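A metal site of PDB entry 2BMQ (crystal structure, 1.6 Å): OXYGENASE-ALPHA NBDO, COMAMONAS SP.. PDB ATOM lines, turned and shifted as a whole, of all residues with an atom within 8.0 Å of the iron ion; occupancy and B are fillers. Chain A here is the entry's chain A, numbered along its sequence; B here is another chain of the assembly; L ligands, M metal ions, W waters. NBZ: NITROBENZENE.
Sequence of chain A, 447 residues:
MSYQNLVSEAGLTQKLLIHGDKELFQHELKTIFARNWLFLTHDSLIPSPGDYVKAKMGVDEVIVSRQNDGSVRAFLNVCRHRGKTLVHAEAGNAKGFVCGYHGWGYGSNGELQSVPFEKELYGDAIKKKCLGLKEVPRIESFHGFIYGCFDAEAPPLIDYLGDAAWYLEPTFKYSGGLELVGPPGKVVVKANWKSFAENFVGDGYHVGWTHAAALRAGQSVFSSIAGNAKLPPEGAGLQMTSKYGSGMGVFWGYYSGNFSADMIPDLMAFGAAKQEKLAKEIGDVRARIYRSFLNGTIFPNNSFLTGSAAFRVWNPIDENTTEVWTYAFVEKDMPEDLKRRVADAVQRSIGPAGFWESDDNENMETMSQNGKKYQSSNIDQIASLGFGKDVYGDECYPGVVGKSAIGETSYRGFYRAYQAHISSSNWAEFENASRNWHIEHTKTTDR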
ATOM      1  N   ASN A 199      32.312   0.508 -29.686  1.00  0.00           N
ATOM      2  CA  ASN A 199      31.625  -0.105 -28.553  1.00  0.00           C
ATOM      3  C   ASN A 199      32.608  -0.500 -27.452  1.00  0.00           C
ATOM      4  O   ASN A 199      32.400  -0.168 -26.284  1.00  0.00           O
ATOM      5  CB  ASN A 199      30.790  -1.291 -29.029  1.00  0.00           C
ATOM      6  CG  ASN A 199      30.034  -1.965 -27.894  1.00  0.00           C
ATOM      7  OD1 ASN A 199      30.527  -2.934 -27.313  1.00  0.00           O
ATOM      8  ND2 ASN A 199      28.846  -1.463 -27.567  1.00  0.00           N
ATOM      9  N   PHE A 200      33.703  -1.155 -27.826  1.00  0.00           N
ATOM     10  CA  PHE A 200      34.673  -1.602 -26.812  1.00  0.00           C
ATOM     11  C   PHE A 200      35.574  -0.479 -26.296  1.00  0.00           C
ATOM     12  O   PHE A 200      36.044  -0.546 -25.155  1.00  0.00           O
ATOM     13  CB  PHE A 200      35.493  -2.820 -27.290  1.00  0.00           C
ATOM     14  CG  PHE A 200      34.821  -4.130 -27.001  1.00  0.00           C
ATOM     15  CD1 PHE A 200      33.633  -4.455 -27.648  1.00  0.00           C
ATOM     16  CD2 PHE A 200      35.342  -5.013 -26.064  1.00  0.00           C
ATOM     17  CE1 PHE A 200      32.968  -5.667 -27.368  1.00  0.00           C
ATOM     18  CE2 PHE A 200      34.695  -6.236 -25.790  1.00  0.00           C
ATOM     19  CZ  PHE A 200      33.489  -6.550 -26.432  1.00  0.00           C
ATOM     20  N   ASP A 203      32.097   2.099 -24.476  1.00  0.00           N
ATOM     21  CA  ASP A 203      30.640   2.031 -24.295  1.00  0.00           C
ATOM     22  C   ASP A 203      30.198   1.425 -22.951  1.00  0.00           C
ATOM     23  O   ASP A 203      29.536   0.389 -22.898  1.00  0.00           O
ATOM     24  CB  ASP A 203      29.956   1.353 -25.484  1.00  0.00           C
ATOM     25  CG  ASP A 203      28.490   1.731 -25.602  1.00  0.00           C
ATOM     26  OD1 ASP A 203      27.899   1.491 -26.681  1.00  0.00           O
ATOM     27  OD2 ASP A 203      27.933   2.274 -24.632  1.00  0.00           O
ATOM     28  N   HIS A 206      26.118   1.368 -22.657  1.00  0.00           N
ATOM     29  CA  HIS A 206      25.197   0.360 -23.233  1.00  0.00           C
ATOM     30  C   HIS A 206      24.921  -0.810 -22.296  1.00  0.00           C
ATOM     31  O   HIS A 206      23.886  -1.457 -22.410  1.00  0.00           O
ATOM     32  CB  HIS A 206      25.659  -0.150 -24.601  1.00  0.00           C
ATOM     33  CG  HIS A 206      26.540  -1.369 -24.554  1.00  0.00           C
ATOM     34  ND1 HIS A 206      27.832  -1.341 -24.082  1.00  0.00           N
ATOM     35  CD2 HIS A 206      26.311  -2.640 -24.954  1.00  0.00           C
ATOM     36  CE1 HIS A 206      28.364  -2.551 -24.180  1.00  0.00           C
ATOM     37  NE2 HIS A 206      27.457  -3.359 -24.711  1.00  0.00           N
ATOM     38  N   VAL A 207      25.858  -1.086 -21.389  1.00  0.00           N
ATOM     39  CA  VAL A 207      25.805  -2.309 -20.586  1.00  0.00           C
ATOM     40  C   VAL A 207      24.470  -2.493 -19.862  1.00  0.00           C
ATOM     41  O   VAL A 207      23.827  -3.538 -19.979  1.00  0.00           O
ATOM     42  CB  VAL A 207      26.975  -2.376 -19.565  1.00  0.00           C
ATOM     43  CG1 VAL A 207      26.875  -3.632 -18.695  1.00  0.00           C
ATOM     44  CG2 VAL A 207      28.299  -2.368 -20.301  1.00  0.00           C
ATOM     45  N   THR A 210      21.327  -2.430 -23.126  1.00  0.00           N
ATOM     46  CA  THR A 210      21.430  -3.541 -24.073  1.00  0.00           C
ATOM     47  C   THR A 210      21.418  -4.900 -23.352  1.00  0.00           C
ATOM     48  O   THR A 210      20.729  -5.835 -23.801  1.00  0.00           O
ATOM     49  CB  THR A 210      22.713  -3.440 -24.916  1.00  0.00           C
ATOM     50  OG1 THR A 210      22.583  -2.373 -25.875  1.00  0.00           O
ATOM     51  CG2 THR A 210      22.984  -4.728 -25.674  1.00  0.00           C
ATOM     52  N   HIS A 211      22.191  -5.001 -22.264  1.00  0.00           N
ATOM     53  CA  HIS A 211      22.375  -6.285 -21.569  1.00  0.00           C
ATOM     54  C   HIS A 211      21.520  -6.445 -20.297  1.00  0.00           C
ATOM     55  O   HIS A 211      21.808  -7.308 -19.463  1.00  0.00           O
ATOM     56  CB  HIS A 211      23.880  -6.511 -21.297  1.00  0.00           C
ATOM     57  CG  HIS A 211      24.711  -6.542 -22.542  1.00  0.00           C
ATOM     58  ND1 HIS A 211      24.493  -7.451 -23.564  1.00  0.00           N
ATOM     59  CD2 HIS A 211      25.753  -5.768 -22.940  1.00  0.00           C
ATOM     60  CE1 HIS A 211      25.379  -7.229 -24.535  1.00  0.00           C
ATOM     61  NE2 HIS A 211      26.143  -6.206 -24.188  1.00  0.00           N
ATOM     62  N   ASN A 258      31.840  -9.255 -17.038  1.00  0.00           N
ATOM     63  CA  ASN A 258      30.585  -9.794 -17.596  1.00  0.00           C
ATOM     64  C   ASN A 258      30.334 -11.263 -17.271  1.00  0.00           C
ATOM     65  O   ASN A 258      29.429 -11.886 -17.836  1.00  0.00           O
ATOM     66  CB  ASN A 258      30.488  -9.513 -19.111  1.00  0.00           C
ATOM     67  CG  ASN A 258      31.536 -10.262 -19.935  1.00  0.00           C
ATOM     68  OD1 ASN A 258      32.017 -11.326 -19.543  1.00  0.00           O
ATOM     69  ND2 ASN A 258      31.882  -9.694 -21.081  1.00  0.00           N
ATOM     70  N   ARG A 312      40.008  -9.326 -28.370  1.00  0.00           N
ATOM     71  CA  ARG A 312      39.167  -9.354 -29.590  1.00  0.00           C
ATOM     72  C   ARG A 312      39.891  -8.754 -30.771  1.00  0.00           C
ATOM     73  O   ARG A 312      40.665  -7.801 -30.611  1.00  0.00           O
ATOM     74  CB  ARG A 312      37.879  -8.533 -29.403  1.00  0.00           C
ATOM     75  CG  ARG A 312      37.147  -8.661 -28.087  1.00  0.00           C
ATOM     76  CD  ARG A 312      36.682 -10.065 -27.817  1.00  0.00           C
ATOM     77  NE  ARG A 312      35.694 -10.625 -28.782  1.00  0.00           N
ATOM     78  CZ  ARG A 312      34.402 -10.311 -28.856  1.00  0.00           C
ATOM     79  NH1 ARG A 312      33.857  -9.367 -28.101  1.00  0.00           N
ATOM     80  NH2 ARG A 312      33.611 -10.943 -29.741  1.00  0.00           N
ATOM     81  N   SER A 349      29.939 -15.519 -22.460  1.00  0.00           N
ATOM     82  CA  SER A 349      29.363 -14.178 -22.549  1.00  0.00           C
ATOM     83  C   SER A 349      29.486 -13.547 -23.935  1.00  0.00           C
ATOM     84  O   SER A 349      28.511 -13.042 -24.473  1.00  0.00           O
ATOM     85  CB  SER A 349      29.979 -13.245 -21.504  1.00  0.00           C
ATOM     86  OG  SER A 349      29.483 -13.570 -20.227  1.00  0.00           O
ATOM     87  N   ILE A 350      30.691 -13.577 -24.528  1.00  0.00           N
ATOM     88  CA  ILE A 350      30.919 -12.782 -25.741  1.00  0.00           C
ATOM     89  C   ILE A 350      31.481 -13.542 -26.945  1.00  0.00           C
ATOM     90  O   ILE A 350      31.828 -12.931 -27.956  1.00  0.00           O
ATOM     91  CB  ILE A 350      31.804 -11.534 -25.454  1.00  0.00           C
ATOM     92  CG1 ILE A 350      33.182 -11.955 -24.971  1.00  0.00           C
ATOM     93  CG2 ILE A 350      31.118 -10.627 -24.436  1.00  0.00           C
ATOM     94  CD1 ILE A 350      34.140 -10.792 -24.722  1.00  0.00           C
ATOM     95  N   TRP A 356      25.662 -12.489 -24.022  1.00  0.00           N
ATOM     96  CA  TRP A 356      25.769 -11.025 -24.067  1.00  0.00           C
ATOM     97  C   TRP A 356      25.979 -10.584 -25.500  1.00  0.00           C
ATOM     98  O   TRP A 356      25.231  -9.759 -26.005  1.00  0.00           O
ATOM     99  CB  TRP A 356      26.941 -10.533 -23.231  1.00  0.00           C
ATOM    100  CG  TRP A 356      26.786 -10.661 -21.745  1.00  0.00           C
ATOM    101  CD1 TRP A 356      26.473 -11.788 -21.034  1.00  0.00           C
ATOM    102  CD2 TRP A 356      27.029  -9.631 -20.774  1.00  0.00           C
ATOM    103  NE1 TRP A 356      26.478 -11.511 -19.673  1.00  0.00           N
ATOM    104  CE2 TRP A 356      26.790 -10.194 -19.497  1.00  0.00           C
ATOM    105  CE3 TRP A 356      27.389  -8.273 -20.875  1.00  0.00           C
ATOM    106  CZ2 TRP A 356      26.937  -9.443 -18.312  1.00  0.00           C
ATOM    107  CZ3 TRP A 356      27.522  -7.531 -19.698  1.00  0.00           C
ATOM    108  CH2 TRP A 356      27.286  -8.123 -18.430  1.00  0.00           C
ATOM    109  N   GLU A 357      27.001 -11.124 -26.164  1.00  0.00           N
ATOM    110  CA  GLU A 357      27.361 -10.565 -27.457  1.00  0.00           C
ATOM    111  C   GLU A 357      26.225 -10.688 -28.472  1.00  0.00           C
ATOM    112  O   GLU A 357      26.104  -9.846 -29.368  1.00  0.00           O
ATOM    113  CB  GLU A 357      28.663 -11.159 -27.992  1.00  0.00           C
ATOM    114  CG  GLU A 357      29.116 -10.443 -29.284  1.00  0.00           C
ATOM    115  CD  GLU A 357      30.582 -10.021 -29.312  1.00  0.00           C
ATOM    116  OE1 GLU A 357      31.072  -9.372 -28.356  1.00  0.00           O
ATOM    117  OE2 GLU A 357      31.240 -10.323 -30.327  1.00  0.00           O
ATOM    118  N   SER A 358      25.377 -11.700 -28.315  1.00  0.00           N
ATOM    119  CA  SER A 358      24.212 -11.868 -29.214  1.00  0.00           C
ATOM    120  C   SER A 358      23.316 -10.636 -29.157  1.00  0.00           C
ATOM    121  O   SER A 358      22.770 -10.235 -30.204  1.00  0.00           O
ATOM    122  CB  SER A 358      23.419 -13.118 -28.857  1.00  0.00           C
ATOM    123  OG  SER A 358      22.946 -13.078 -27.528  1.00  0.00           O
ATOM    124  N   ASP A 359      23.172 -10.042 -27.968  1.00  0.00           N
ATOM    125  CA  ASP A 359      22.414  -8.804 -27.769  1.00  0.00           C
ATOM    126  C   ASP A 359      22.972  -7.715 -28.696  1.00  0.00           C
ATOM    127  O   ASP A 359      22.214  -6.930 -29.282  1.00  0.00           O
ATOM    128  CB  ASP A 359      22.518  -8.260 -26.334  1.00  0.00           C
ATOM    129  CG  ASP A 359      21.919  -9.211 -25.261  1.00  0.00           C
ATOM    130  OD1 ASP A 359      22.411  -9.187 -24.103  1.00  0.00           O
ATOM    131  OD2 ASP A 359      20.962  -9.952 -25.571  1.00  0.00           O
ATOM    132  N   ASP A 360      24.296  -7.669 -28.796  1.00  0.00           N
ATOM    133  CA  ASP A 360      24.993  -6.583 -29.488  1.00  0.00           C
ATOM    134  C   ASP A 360      24.856  -6.600 -30.997  1.00  0.00           C
ATOM    135  O   ASP A 360      24.969  -5.564 -31.643  1.00  0.00           O
ATOM    136  CB  ASP A 360      26.472  -6.612 -29.138  1.00  0.00           C
ATOM    137  CG  ASP A 360      26.745  -6.177 -27.717  1.00  0.00           C
ATOM    138  OD1 ASP A 360      26.277  -5.079 -27.330  1.00  0.00           O
ATOM    139  OD2 ASP A 360      27.399  -6.937 -26.992  1.00  0.00           O
ATOM    140  N   ASN A 361      24.590  -7.769 -31.561  1.00  0.00           N
ATOM    141  CA  ASN A 361      24.536  -7.904 -33.006  1.00  0.00           C
ATOM    142  C   ASN A 361      23.679  -6.830 -33.632  1.00  0.00           C
ATOM    143  O   ASN A 361      24.107  -6.167 -34.565  1.00  0.00           O
ATOM    144  CB  ASN A 361      23.999  -9.268 -33.463  1.00  0.00           C
ATOM    145  CG  ASN A 361      24.961 -10.415 -33.238  1.00  0.00           C
ATOM    146  OD1 ASN A 361      26.132 -10.242 -32.864  1.00  0.00           O
ATOM    147  ND2 ASN A 361      24.449 -11.621 -33.456  1.00  0.00           N
ATOM    148  N   ASN A 363      22.643  -3.987 -32.516  1.00  0.00           N
ATOM    149  CA  ASN A 363      23.186  -2.632 -32.328  1.00  0.00           C
ATOM    150  C   ASN A 363      24.174  -2.307 -33.448  1.00  0.00           C
ATOM    151  O   ASN A 363      24.041  -1.281 -34.140  1.00  0.00           O
ATOM    152  CB  ASN A 363      23.885  -2.480 -30.968  1.00  0.00           C
ATOM    153  CG  ASN A 363      22.933  -2.656 -29.790  1.00  0.00           C
ATOM    154  OD1 ASN A 363      21.717  -2.479 -29.913  1.00  0.00           O
ATOM    155  ND2 ASN A 363      23.495  -2.980 -28.624  1.00  0.00           N
ATOM    156  N   MET A 364      25.169  -3.184 -33.588  1.00  0.00           N
ATOM    157  CA  MET A 364      26.271  -3.043 -34.540  1.00  0.00           C
ATOM    158  C   MET A 364      25.800  -3.102 -35.986  1.00  0.00           C
ATOM    159  O   MET A 364      26.127  -2.250 -36.808  1.00  0.00           O
ATOM    160  CB  MET A 364      27.298  -4.165 -34.324  1.00  0.00           C
ATOM    161  CG  MET A 364      27.824  -4.344 -32.905  1.00  0.00           C
ATOM    162  SD  MET A 364      28.965  -3.034 -32.408  1.00  0.00           S
ATOM    163  CE  MET A 364      27.830  -1.973 -31.524  1.00  0.00           C
ATOM    164  N   TYR B 101      19.703   0.260 -27.673  1.00  0.00           N
ATOM    165  CA  TYR B 101      21.158   0.343 -27.479  1.00  0.00           C
ATOM    166  C   TYR B 101      21.504   0.964 -26.124  1.00  0.00           C
ATOM    167  O   TYR B 101      22.010   0.269 -25.236  1.00  0.00           O
ATOM    168  CB  TYR B 101      21.819   1.094 -28.651  1.00  0.00           C
ATOM    169  CG  TYR B 101      23.296   0.837 -28.856  1.00  0.00           C
ATOM    170  CD1 TYR B 101      23.930   1.300 -30.013  1.00  0.00           C
ATOM    171  CD2 TYR B 101      24.070   0.157 -27.912  1.00  0.00           C
ATOM    172  CE1 TYR B 101      25.297   1.089 -30.231  1.00  0.00           C
ATOM    173  CE2 TYR B 101      25.459  -0.052 -28.129  1.00  0.00           C
ATOM    174  CZ  TYR B 101      26.052   0.417 -29.290  1.00  0.00           C
ATOM    175  OH  TYR B 101      27.409   0.223 -29.537  1.00  0.00           O
HETATM  176  C1  NBZ L   1      31.494  -3.763 -21.514  1.00  0.00           C
HETATM  177  C2  NBZ L   1      31.822  -2.514 -22.059  1.00  0.00           C
HETATM  178  C3  NBZ L   1      32.098  -2.406 -23.424  1.00  0.00           C
HETATM  179  C4  NBZ L   1      32.046  -3.541 -24.235  1.00  0.00           C
HETATM  180  C5  NBZ L   1      31.722  -4.781 -23.694  1.00  0.00           C
HETATM  181  C6  NBZ L   1      31.442  -4.898 -22.325  1.00  0.00           C
HETATM  182  N1  NBZ L   1      31.129  -6.097 -21.758  1.00  0.00           N
HETATM  183  O1  NBZ L   1      30.952  -7.123 -22.445  1.00  0.00           O
HETATM  184  O2  NBZ L   1      30.980  -6.163 -20.516  1.00  0.00           O
HETATM  185 FE    FE M   1      27.656  -5.381 -25.386  1.00  0.00          FE
HETATM  186  O   HOH W   1      29.000  -7.042 -24.289  1.00  0.00           O
HETATM  187  O   HOH W   2      29.639  -5.006 -26.314  1.00  0.00           O
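ND2 of Asn 258 is in hydrogen-bond range of O1 of the ligand (3.1 Å).
The iron ion is bound by a ring nitrogen (NE2) of His 211, a ring nitrogen (NE2) of His 206, water W2, the side-chain carboxylate (OD2) of Asp 360, the side-chain carboxylate (OD1) of Asp 360 and water W1.
The iron ion has six donor atoms within binding distance.
A ring nitrogen (ND1) of His 211 sits close to the backbone carbonyl oxygen of Trp 356.
A ring nitrogen (ND1) of His 206 is in hydrogen-bond range of the backbone carbonyl oxygen (O) of Asp 203, 2.7 Å away.
The side-chain carboxylate (OD1) of Asp 359 lies within hydrogen-bond range of a ring nitrogen (ND1) of His 211 (2.8 Å).
Within 4 Å of the iron ion: His 206, His 211 and Asp 360.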
